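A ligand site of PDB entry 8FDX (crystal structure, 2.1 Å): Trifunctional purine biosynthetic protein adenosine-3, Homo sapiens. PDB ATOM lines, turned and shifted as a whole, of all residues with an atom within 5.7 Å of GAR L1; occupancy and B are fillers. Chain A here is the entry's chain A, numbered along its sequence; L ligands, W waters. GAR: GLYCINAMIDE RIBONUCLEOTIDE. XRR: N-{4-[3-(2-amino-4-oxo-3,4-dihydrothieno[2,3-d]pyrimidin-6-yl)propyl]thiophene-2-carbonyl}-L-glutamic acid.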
ATOM      1  N   GLY A  10     -18.529   5.903 -12.834  1.00  0.00           N
ATOM      2  CA  GLY A  10     -18.113   7.153 -13.446  1.00  0.00           C
ATOM      3  C   GLY A  10     -19.137   7.850 -14.324  1.00  0.00           C
ATOM      4  O   GLY A  10     -20.261   8.119 -13.873  1.00  0.00           O
ATOM      5  N   THR A  11     -18.763   8.125 -15.576  1.00  0.00           N
ATOM      6  CA  THR A  11     -19.565   9.011 -16.418  1.00  0.00           C
ATOM      7  C   THR A  11     -20.946   8.427 -16.716  1.00  0.00           C
ATOM      8  O   THR A  11     -21.955   9.146 -16.712  1.00  0.00           O
ATOM      9  CB  THR A  11     -18.849   9.285 -17.740  1.00  0.00           C
ATOM     10  OG1 THR A  11     -17.614   9.973 -17.481  1.00  0.00           O
ATOM     11  CG2 THR A  11     -19.734  10.124 -18.643  1.00  0.00           C
ATOM     12  N   GLY A  12     -21.008   7.146 -17.045  1.00  0.00           N
ATOM     13  CA  GLY A  12     -22.293   6.492 -17.221  1.00  0.00           C
ATOM     14  C   GLY A  12     -22.889   6.583 -18.612  1.00  0.00           C
ATOM     15  O   GLY A  12     -24.111   6.509 -18.745  1.00  0.00           O
ATOM     16  N   SER A  13     -22.059   6.737 -19.653  1.00  0.00           N
ATOM     17  CA  SER A  13     -22.599   6.721 -21.007  1.00  0.00           C
ATOM     18  C   SER A  13     -23.153   5.346 -21.382  1.00  0.00           C
ATOM     19  O   SER A  13     -24.148   5.262 -22.107  1.00  0.00           O
ATOM     20  CB  SER A  13     -21.545   7.180 -22.025  1.00  0.00           C
ATOM     21  OG  SER A  13     -20.423   6.328 -22.077  1.00  0.00           O
ATOM     22  N   ASN A  14     -22.541   4.255 -20.895  1.00  0.00           N
ATOM     23  CA  ASN A  14     -23.138   2.936 -21.114  1.00  0.00           C
ATOM     24  C   ASN A  14     -24.454   2.788 -20.377  1.00  0.00           C
ATOM     25  O   ASN A  14     -25.412   2.221 -20.908  1.00  0.00           O
ATOM     26  CB  ASN A  14     -22.184   1.835 -20.676  1.00  0.00           C
ATOM     27  CG  ASN A  14     -21.200   1.493 -21.741  1.00  0.00           C
ATOM     28  OD1 ASN A  14     -21.556   0.871 -22.747  1.00  0.00           O
ATOM     29  ND2 ASN A  14     -19.950   1.911 -21.560  1.00  0.00           N
ATOM     30  N   LEU A  15     -24.520   3.273 -19.138  1.00  0.00           N
ATOM     31  CA  LEU A  15     -25.793   3.337 -18.431  1.00  0.00           C
ATOM     32  C   LEU A  15     -26.851   4.029 -19.278  1.00  0.00           C
ATOM     33  O   LEU A  15     -27.969   3.528 -19.434  1.00  0.00           O
ATOM     34  CB  LEU A  15     -25.630   4.057 -17.102  1.00  0.00           C
ATOM     35  CG  LEU A  15     -26.986   4.438 -16.492  1.00  0.00           C
ATOM     36  CD1 LEU A  15     -27.809   3.170 -16.106  1.00  0.00           C
ATOM     37  CD2 LEU A  15     -26.815   5.377 -15.296  1.00  0.00           C
ATOM     38  N   ALA A  87     -21.327  -1.450 -15.906  1.00  0.00           N
ATOM     39  CA  ALA A  87     -21.223  -0.450 -16.963  1.00  0.00           C
ATOM     40  C   ALA A  87     -20.231   0.608 -16.501  1.00  0.00           C
ATOM     41  O   ALA A  87     -20.608   1.618 -15.881  1.00  0.00           O
ATOM     42  CB  ALA A  87     -22.598   0.141 -17.291  1.00  0.00           C
ATOM     43  N   GLY A  88     -18.957   0.388 -16.798  1.00  0.00           N
ATOM     44  CA  GLY A  88     -17.927   1.265 -16.279  1.00  0.00           C
ATOM     45  C   GLY A  88     -17.657   1.097 -14.808  1.00  0.00           C
ATOM     46  O   GLY A  88     -16.971   1.925 -14.211  1.00  0.00           O
ATOM     47  N   PHE A  89     -18.225   0.060 -14.183  1.00  0.00           N
ATOM     48  CA  PHE A  89     -17.920  -0.249 -12.797  1.00  0.00           C
ATOM     49  C   PHE A  89     -16.519  -0.832 -12.709  1.00  0.00           C
ATOM     50  O   PHE A  89     -16.176  -1.769 -13.440  1.00  0.00           O
ATOM     51  CB  PHE A  89     -18.952  -1.227 -12.258  1.00  0.00           C
ATOM     52  CG  PHE A  89     -18.727  -1.648 -10.844  1.00  0.00           C
ATOM     53  CD1 PHE A  89     -19.118  -0.832  -9.800  1.00  0.00           C
ATOM     54  CD2 PHE A  89     -18.134  -2.871 -10.560  1.00  0.00           C
ATOM     55  CE1 PHE A  89     -18.928  -1.231  -8.489  1.00  0.00           C
ATOM     56  CE2 PHE A  89     -17.927  -3.275  -9.266  1.00  0.00           C
ATOM     57  CZ  PHE A  89     -18.331  -2.460  -8.218  1.00  0.00           C
ATOM     58  N   MET A  90     -15.703  -0.304 -11.798  1.00  0.00           N
ATOM     59  CA  MET A  90     -14.258  -0.516 -11.865  1.00  0.00           C
ATOM     60  C   MET A  90     -13.686  -1.359 -10.733  1.00  0.00           C
ATOM     61  O   MET A  90     -12.466  -1.541 -10.683  1.00  0.00           O
ATOM     62  CB  MET A  90     -13.532   0.844 -11.885  1.00  0.00           C
ATOM     63  CG  MET A  90     -13.409   1.491 -13.280  1.00  0.00           C
ATOM     64  SD  MET A  90     -13.187   0.368 -14.703  1.00  0.00           S
ATOM     65  CE  MET A  90     -11.709  -0.550 -14.243  1.00  0.00           C
ATOM     66  N   ASN A 107     -20.547  -7.726 -18.161  1.00  0.00           N
ATOM     67  CA  ASN A 107     -19.561  -6.659 -18.130  1.00  0.00           C
ATOM     68  C   ASN A 107     -19.283  -6.189 -19.547  1.00  0.00           C
ATOM     69  O   ASN A 107     -19.300  -6.994 -20.488  1.00  0.00           O
ATOM     70  CB  ASN A 107     -18.276  -7.133 -17.479  1.00  0.00           C
ATOM     71  CG  ASN A 107     -17.230  -6.054 -17.467  1.00  0.00           C
ATOM     72  OD1 ASN A 107     -17.495  -4.938 -17.032  1.00  0.00           O
ATOM     73  ND2 ASN A 107     -16.042  -6.374 -17.964  1.00  0.00           N
ATOM     74  N   ILE A 108     -19.062  -4.893 -19.712  1.00  0.00           N
ATOM     75  CA  ILE A 108     -18.632  -4.309 -20.980  1.00  0.00           C
ATOM     76  C   ILE A 108     -17.165  -3.941 -20.853  1.00  0.00           C
ATOM     77  O   ILE A 108     -16.760  -3.286 -19.871  1.00  0.00           O
ATOM     78  CB  ILE A 108     -19.512  -3.103 -21.372  1.00  0.00           C
ATOM     79  CG1 ILE A 108     -19.061  -2.512 -22.710  1.00  0.00           C
ATOM     80  CG2 ILE A 108     -19.500  -2.011 -20.292  1.00  0.00           C
ATOM     81  CD1 ILE A 108     -19.164  -3.445 -23.853  1.00  0.00           C
ATOM     82  N   HIS A 109     -16.347  -4.422 -21.790  1.00  0.00           N
ATOM     83  CA  HIS A 109     -14.908  -4.218 -21.740  1.00  0.00           C
ATOM     84  C   HIS A 109     -14.451  -3.614 -23.058  1.00  0.00           C
ATOM     85  O   HIS A 109     -14.785  -4.151 -24.138  1.00  0.00           O
ATOM     86  CB  HIS A 109     -14.167  -5.541 -21.459  1.00  0.00           C
ATOM     87  CG  HIS A 109     -12.682  -5.363 -21.342  1.00  0.00           C
ATOM     88  ND1 HIS A 109     -12.074  -4.877 -20.207  1.00  0.00           N
ATOM     89  CD2 HIS A 109     -11.685  -5.600 -22.224  1.00  0.00           C
ATOM     90  CE1 HIS A 109     -10.760  -4.829 -20.391  1.00  0.00           C
ATOM     91  NE2 HIS A 109     -10.503  -5.272 -21.606  1.00  0.00           N
ATOM     92  N   PRO A 110     -13.657  -2.504 -23.034  1.00  0.00           N
ATOM     93  CA  PRO A 110     -13.299  -1.766 -24.236  1.00  0.00           C
ATOM     94  C   PRO A 110     -12.120  -2.374 -25.005  1.00  0.00           C
ATOM     95  O   PRO A 110     -11.188  -1.669 -25.405  1.00  0.00           O
ATOM     96  CB  PRO A 110     -12.962  -0.385 -23.705  1.00  0.00           C
ATOM     97  CG  PRO A 110     -12.362  -0.649 -22.360  1.00  0.00           C
ATOM     98  CD  PRO A 110     -13.039  -1.904 -21.821  1.00  0.00           C
ATOM     99  N   GLY A 118      -7.823  -5.959 -18.453  1.00  0.00           N
ATOM    100  CA  GLY A 118      -7.366  -4.990 -17.475  1.00  0.00           C
ATOM    101  C   GLY A 118      -7.955  -3.605 -17.664  1.00  0.00           C
ATOM    102  O   GLY A 118      -8.859  -3.371 -18.479  1.00  0.00           O
ATOM    103  N   SER A 119      -7.404  -2.668 -16.909  1.00  0.00           N
ATOM    104  CA  SER A 119      -8.074  -1.389 -16.657  1.00  0.00           C
ATOM    105  C   SER A 119      -7.812  -0.326 -17.718  1.00  0.00           C
ATOM    106  O   SER A 119      -8.502   0.705 -17.721  1.00  0.00           O
ATOM    107  CB  SER A 119      -7.635  -0.845 -15.294  1.00  0.00           C
ATOM    108  OG  SER A 119      -6.229  -0.947 -15.182  1.00  0.00           O
ATOM    109  N   ASN A 120      -6.836  -0.529 -18.591  1.00  0.00           N
ATOM    110  CA  ASN A 120      -6.388   0.476 -19.549  1.00  0.00           C
ATOM    111  C   ASN A 120      -6.277  -0.121 -20.949  1.00  0.00           C
ATOM    112  O   ASN A 120      -5.234  -0.042 -21.601  1.00  0.00           O
ATOM    113  CB  ASN A 120      -5.047   1.022 -19.082  1.00  0.00           C
ATOM    114  CG  ASN A 120      -4.027  -0.091 -18.951  1.00  0.00           C
ATOM    115  OD1 ASN A 120      -4.399  -1.243 -18.715  1.00  0.00           O
ATOM    116  ND2 ASN A 120      -2.744   0.244 -19.104  1.00  0.00           N
ATOM    117  N   HIS A 122      -7.363   0.666 -23.847  1.00  0.00           N
ATOM    118  CA  HIS A 122      -7.027   1.565 -24.944  1.00  0.00           C
ATOM    119  C   HIS A 122      -5.529   1.863 -24.970  1.00  0.00           C
ATOM    120  O   HIS A 122      -4.897   1.783 -26.027  1.00  0.00           O
ATOM    121  CB  HIS A 122      -7.820   2.852 -24.842  1.00  0.00           C
ATOM    122  CG  HIS A 122      -9.294   2.653 -24.954  1.00  0.00           C
ATOM    123  ND1 HIS A 122      -9.870   1.969 -26.008  1.00  0.00           N
ATOM    124  CD2 HIS A 122     -10.305   3.008 -24.132  1.00  0.00           C
ATOM    125  CE1 HIS A 122     -11.175   1.936 -25.836  1.00  0.00           C
ATOM    126  NE2 HIS A 122     -11.466   2.564 -24.713  1.00  0.00           N
ATOM    127  N   ASP A 145     -12.212 -10.436 -16.769  1.00  0.00           N
ATOM    128  CA  ASP A 145     -12.232 -10.266 -18.227  1.00  0.00           C
ATOM    129  C   ASP A 145     -12.041 -11.593 -18.959  1.00  0.00           C
ATOM    130  O   ASP A 145     -11.498 -11.621 -20.077  1.00  0.00           O
ATOM    131  CB  ASP A 145     -11.173  -9.257 -18.699  1.00  0.00           C
ATOM    132  CG  ASP A 145     -11.409  -7.860 -18.137  1.00  0.00           C
ATOM    133  OD1 ASP A 145     -12.559  -7.543 -17.758  1.00  0.00           O
ATOM    134  OD2 ASP A 145     -10.426  -7.079 -18.084  1.00  0.00           O
ATOM    135  N   LYS A 171     -16.721   3.646 -27.731  1.00  0.00           N
ATOM    136  CA  LYS A 171     -17.952   3.791 -26.969  1.00  0.00           C
ATOM    137  C   LYS A 171     -19.170   3.808 -27.877  1.00  0.00           C
ATOM    138  O   LYS A 171     -20.257   3.399 -27.456  1.00  0.00           O
ATOM    139  CB  LYS A 171     -17.874   5.038 -26.089  1.00  0.00           C
ATOM    140  CG  LYS A 171     -17.082   4.795 -24.816  1.00  0.00           C
ATOM    141  CD  LYS A 171     -17.180   5.962 -23.831  1.00  0.00           C
ATOM    142  CE  LYS A 171     -16.434   5.601 -22.541  1.00  0.00           C
ATOM    143  NZ  LYS A 171     -16.574   6.637 -21.458  1.00  0.00           N
ATOM    144  N   GLU A 174     -19.784   0.213 -28.082  1.00  0.00           N
ATOM    145  CA  GLU A 174     -20.222  -0.247 -26.770  1.00  0.00           C
ATOM    146  C   GLU A 174     -21.711  -0.012 -26.581  1.00  0.00           C
ATOM    147  O   GLU A 174     -22.435  -0.894 -26.104  1.00  0.00           O
ATOM    148  CB  GLU A 174     -19.432   0.485 -25.687  1.00  0.00           C
ATOM    149  CG  GLU A 174     -18.096  -0.151 -25.350  1.00  0.00           C
ATOM    150  CD  GLU A 174     -17.358   0.651 -24.276  1.00  0.00           C
ATOM    151  OE1 GLU A 174     -16.226   1.152 -24.514  1.00  0.00           O
ATOM    152  OE2 GLU A 174     -17.944   0.816 -23.196  1.00  0.00           O
ATOM    153  N   HIS A 175     -22.183   1.176 -26.981  1.00  0.00           N
ATOM    154  CA  HIS A 175     -23.577   1.543 -26.792  1.00  0.00           C
ATOM    155  C   HIS A 175     -24.502   0.821 -27.736  1.00  0.00           C
ATOM    156  O   HIS A 175     -25.722   0.973 -27.609  1.00  0.00           O
ATOM    157  CB  HIS A 175     -23.761   3.050 -26.968  1.00  0.00           C
ATOM    158  CG  HIS A 175     -22.937   3.859 -26.017  1.00  0.00           C
ATOM    159  ND1 HIS A 175     -22.511   5.144 -26.292  1.00  0.00           N
ATOM    160  CD2 HIS A 175     -22.434   3.545 -24.802  1.00  0.00           C
ATOM    161  CE1 HIS A 175     -21.799   5.595 -25.278  1.00  0.00           C
ATOM    162  NE2 HIS A 175     -21.727   4.643 -24.360  1.00  0.00           N
HETATM  163  C1  GAR L   1     -16.352   2.173 -20.852  1.00  0.00           C
HETATM  164  O6  GAR L   1     -15.509   2.332 -22.013  1.00  0.00           O
HETATM  165  C2  GAR L   1     -16.159   0.771 -20.324  1.00  0.00           C
HETATM  166  O8  GAR L   1     -15.999  -0.219 -21.357  1.00  0.00           O
HETATM  167  C3  GAR L   1     -14.869   0.946 -19.541  1.00  0.00           C
HETATM  168  O4  GAR L   1     -14.985   2.223 -18.933  1.00  0.00           O
HETATM  169  C5  GAR L   1     -15.822   3.056 -19.736  1.00  0.00           C
HETATM  170  C10 GAR L   1     -16.935   3.601 -18.866  1.00  0.00           C
HETATM  171  O12 GAR L   1     -17.704   4.570 -19.565  1.00  0.00           O
HETATM  172  N19 GAR L   1     -14.744  -0.070 -18.519  1.00  0.00           N
HETATM  173  C21 GAR L   1     -13.606  -0.719 -18.360  1.00  0.00           C
HETATM  174  O22 GAR L   1     -12.500  -0.263 -18.667  1.00  0.00           O
HETATM  175  C23 GAR L   1     -13.772  -2.107 -17.766  1.00  0.00           C
HETATM  176  N24 GAR L   1     -12.503  -2.673 -17.369  1.00  0.00           N
HETATM  177  P15 GAR L   1     -19.148   5.029 -19.005  1.00  0.00           P
HETATM  178  O16 GAR L   1     -20.079   3.869 -19.325  1.00  0.00           O
HETATM  179  O17 GAR L   1     -19.428   6.290 -19.810  1.00  0.00           O
HETATM  180  O18 GAR L   1     -18.963   5.218 -17.511  1.00  0.00           O
HETATM  181  O10 XRR L   2     -14.569 -10.204 -15.094  1.00  0.00           O
HETATM  182  N11 XRR L   2     -14.236 -11.611 -10.508  1.00  0.00           N
HETATM  183  C14 XRR L   2     -11.359  -3.747 -13.035  1.00  0.00           C
HETATM  184  C15 XRR L   2     -10.644  -4.776 -15.056  1.00  0.00           C
HETATM  185  C17 XRR L   2      -9.215  -2.869 -11.763  1.00  0.00           C
HETATM  186  O18 XRR L   2      -8.037  -2.731 -11.822  1.00  0.00           O
HETATM  187  N19 XRR L   2      -9.937  -2.448 -10.587  1.00  0.00           N
HETATM  188  C20 XRR L   2      -9.241  -1.829  -9.472  1.00  0.00           C
HETATM  189  C21 XRR L   2      -9.752  -0.408  -9.229  1.00  0.00           C
HETATM  190  C22 XRR L   2      -9.254   0.573 -10.290  1.00  0.00           C
HETATM  191  C23 XRR L   2     -10.218   1.753 -10.508  1.00  0.00           C
HETATM  192  O24 XRR L   2     -10.256   2.341 -11.633  1.00  0.00           O
HETATM  193  O25 XRR L   2     -10.969   2.137  -9.569  1.00  0.00           O
HETATM  194  C26 XRR L   2      -9.500  -2.715  -8.250  1.00  0.00           C
HETATM  195  O27 XRR L   2      -8.634  -2.803  -7.338  1.00  0.00           O
HETATM  196  O28 XRR L   2     -10.575  -3.386  -8.149  1.00  0.00           O
HETATM  197  C29 XRR L   2     -15.605  -4.827 -14.267  1.00  0.00           C
HETATM  198  C30 XRR L   2     -14.308  -4.045 -14.001  1.00  0.00           C
HETATM  199  C31 XRR L   2     -13.163  -4.800 -14.654  1.00  0.00           C
HETATM  200  C32 XRR L   2     -11.737  -4.431 -14.239  1.00  0.00           C
HETATM  201  C02 XRR L   2     -14.454 -10.607 -11.522  1.00  0.00           C
HETATM  202  C04 XRR L   2     -14.601  -9.938 -13.934  1.00  0.00           C
HETATM  203  C05 XRR L   2     -15.115  -7.418 -14.390  1.00  0.00           C
HETATM  204  C06 XRR L   2     -15.364  -6.224 -13.702  1.00  0.00           C
HETATM  205  C08 XRR L   2     -14.890  -8.533 -13.492  1.00  0.00           C
HETATM  206  C09 XRR L   2     -14.936  -8.214 -12.134  1.00  0.00           C
HETATM  207  C12 XRR L   2      -9.969  -3.538 -12.905  1.00  0.00           C
HETATM  208  N01 XRR L   2     -14.721  -9.240 -11.110  1.00  0.00           N
HETATM  209  N03 XRR L   2     -14.395 -10.948 -12.938  1.00  0.00           N
HETATM  210  S07 XRR L   2     -15.275  -6.573 -12.048  1.00  0.00           S
HETATM  211  S13 XRR L   2      -9.245  -4.227 -14.270  1.00  0.00           S
HETATM  212  O   HOH W   1     -21.866   3.300 -17.484  1.00  0.00           O
HETATM  213  O   HOH W   2     -13.441   3.262 -16.787  1.00  0.00           O
HETATM  214  O   HOH W   3     -17.246  -1.554 -18.074  1.00  0.00           O
HETATM  215  O   HOH W   4     -16.546   6.179 -16.575  1.00  0.00           O
HETATM  216  O   HOH W   5     -12.956   3.362 -22.118  1.00  0.00           O
HETATM  217  O   HOH W   6     -19.305   4.173 -15.009  1.00  0.00           O
HETATM  218  O   HOH W   7      -9.753  -1.203 -19.954  1.00  0.00           O
HETATM  219  O   HOH W   8     -13.391  -5.198 -17.985  1.00  0.00           O
HETATM  220  O   HOH W   9     -14.319   3.283 -25.001  1.00  0.00           O
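The side-chain carboxylate of Glu 174 lies within hydrogen-bond range of an oxygen (O6) of GAR L1. The backbone NH of Thr 11 lies within hydrogen-bond range of an oxygen (O18) of GAR L1. O of Ile 108 lies within hydrogen-bond range of O8 of GAR L1. The side-chain hydroxyl (OG) of Ser 13 is in hydrogen-bond range of an oxygen (O17) of GAR L1 (2.5 Å). N of Ser 119 lies close to S13 of XRR L2 (3.6 Å). An oxygen (O16) of GAR L1 is in hydrogen-bond range of the side-chain amide nitrogen (ND2) of Asn 14, at 3.0 Å. An oxygen (O17) of GAR L1 sits at hydrogen-bond distance from the backbone NH of Ser 13. The backbone NH (N) of Asn 14 is in hydrogen-bond range of an oxygen (O16) of GAR L1 (2.9 Å). N of Asp 145 sits at hydrogen-bond distance from O10 of XRR L2, at 2.9 Å. The side-chain amino group of Lys 171 lies within salt-bridge range of an oxygen (O17) of GAR L1 (3.3 Å). An oxygen (O18) of GAR L1 sits at hydrogen-bond distance from the backbone NH (N) of Gly 12, at 2.8 Å. O of Met 90 is in hydrogen-bond range of N19 of XRR L2 (2.7 Å).
OE2 of Glu 174 lies within hydrogen-bond range of ND2 of Asn 14, 2.8 Å away. A ring nitrogen (ND1) of His 109 lies close to the side-chain carboxylate (OD2) of Asp 145, 3.5 Å away. The side-chain hydroxyl of Ser 13 is in hydrogen-bond range of a ring nitrogen (NE2) of His 175 (3.1 Å). The backbone NH of Gly 118 is in hydrogen-bond range of the side-chain carboxylate of Asp 145. The backbone carbonyl oxygen (O) of Lys 171 lies close to a ring nitrogen (ND1) of His 175 (3.1 Å).
CA of Gly 88 touches C10 of GAR L1, 3.6 Å away. SD of Met 90 touches C21 of GAR L1, at 3.8 Å. His 109 touches GAR L1 (ND1 to N24, 3.6 Å). Pro 110 touches GAR L1 (CD to O8, 3.4 Å). O of Gly 118 touches N24 of GAR L1 (3.9 Å). Hydrophobic or aromatic side chains within 4 Å of GAR L1: Met 90 and Pro 110. 12 residues have an atom within 4 Å of GAR L1: Thr 11, Gly 12, Ser 13, Asn 14, Gly 88, Met 90, Ile 108, His 109, Pro 110, Gly 118, Lys 171 and Glu 174. Along chain A the residues within 4 Å of GAR L1 span positions 11 to 174. The nearest printed residue that does not touch GAR L1 is Gly 10 (4.1 Å).
Water W1 lies within hydrogen-bond range of O16 of GAR L1, O of Ala 87 and N of Leu 15. Water W8 lies within hydrogen-bond range of OD1 of Asp 145 (2.5 Å), ND1 of His 109 (2.6 Å), N24 of GAR L1 (2.7 Å) and ND2 of Asn 107 (2.9 Å). Water W4 lies within hydrogen-bond range of an oxygen (O18) of GAR L1 and the backbone NH (N) of Thr 11. Water W2 lies within hydrogen-bond range of an oxygen (O4) of GAR L1 (2.8 Å) and the side-chain sulfur (SD) of Met 90 (3.6 Å). Water W3 lies within hydrogen-bond range of O of Ile 108, N of Gly 88 and N19 of GAR L1. Water W9 lies within hydrogen-bond range of OE1 of Glu 174, NE2 of His 122 and O6 of GAR L1.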
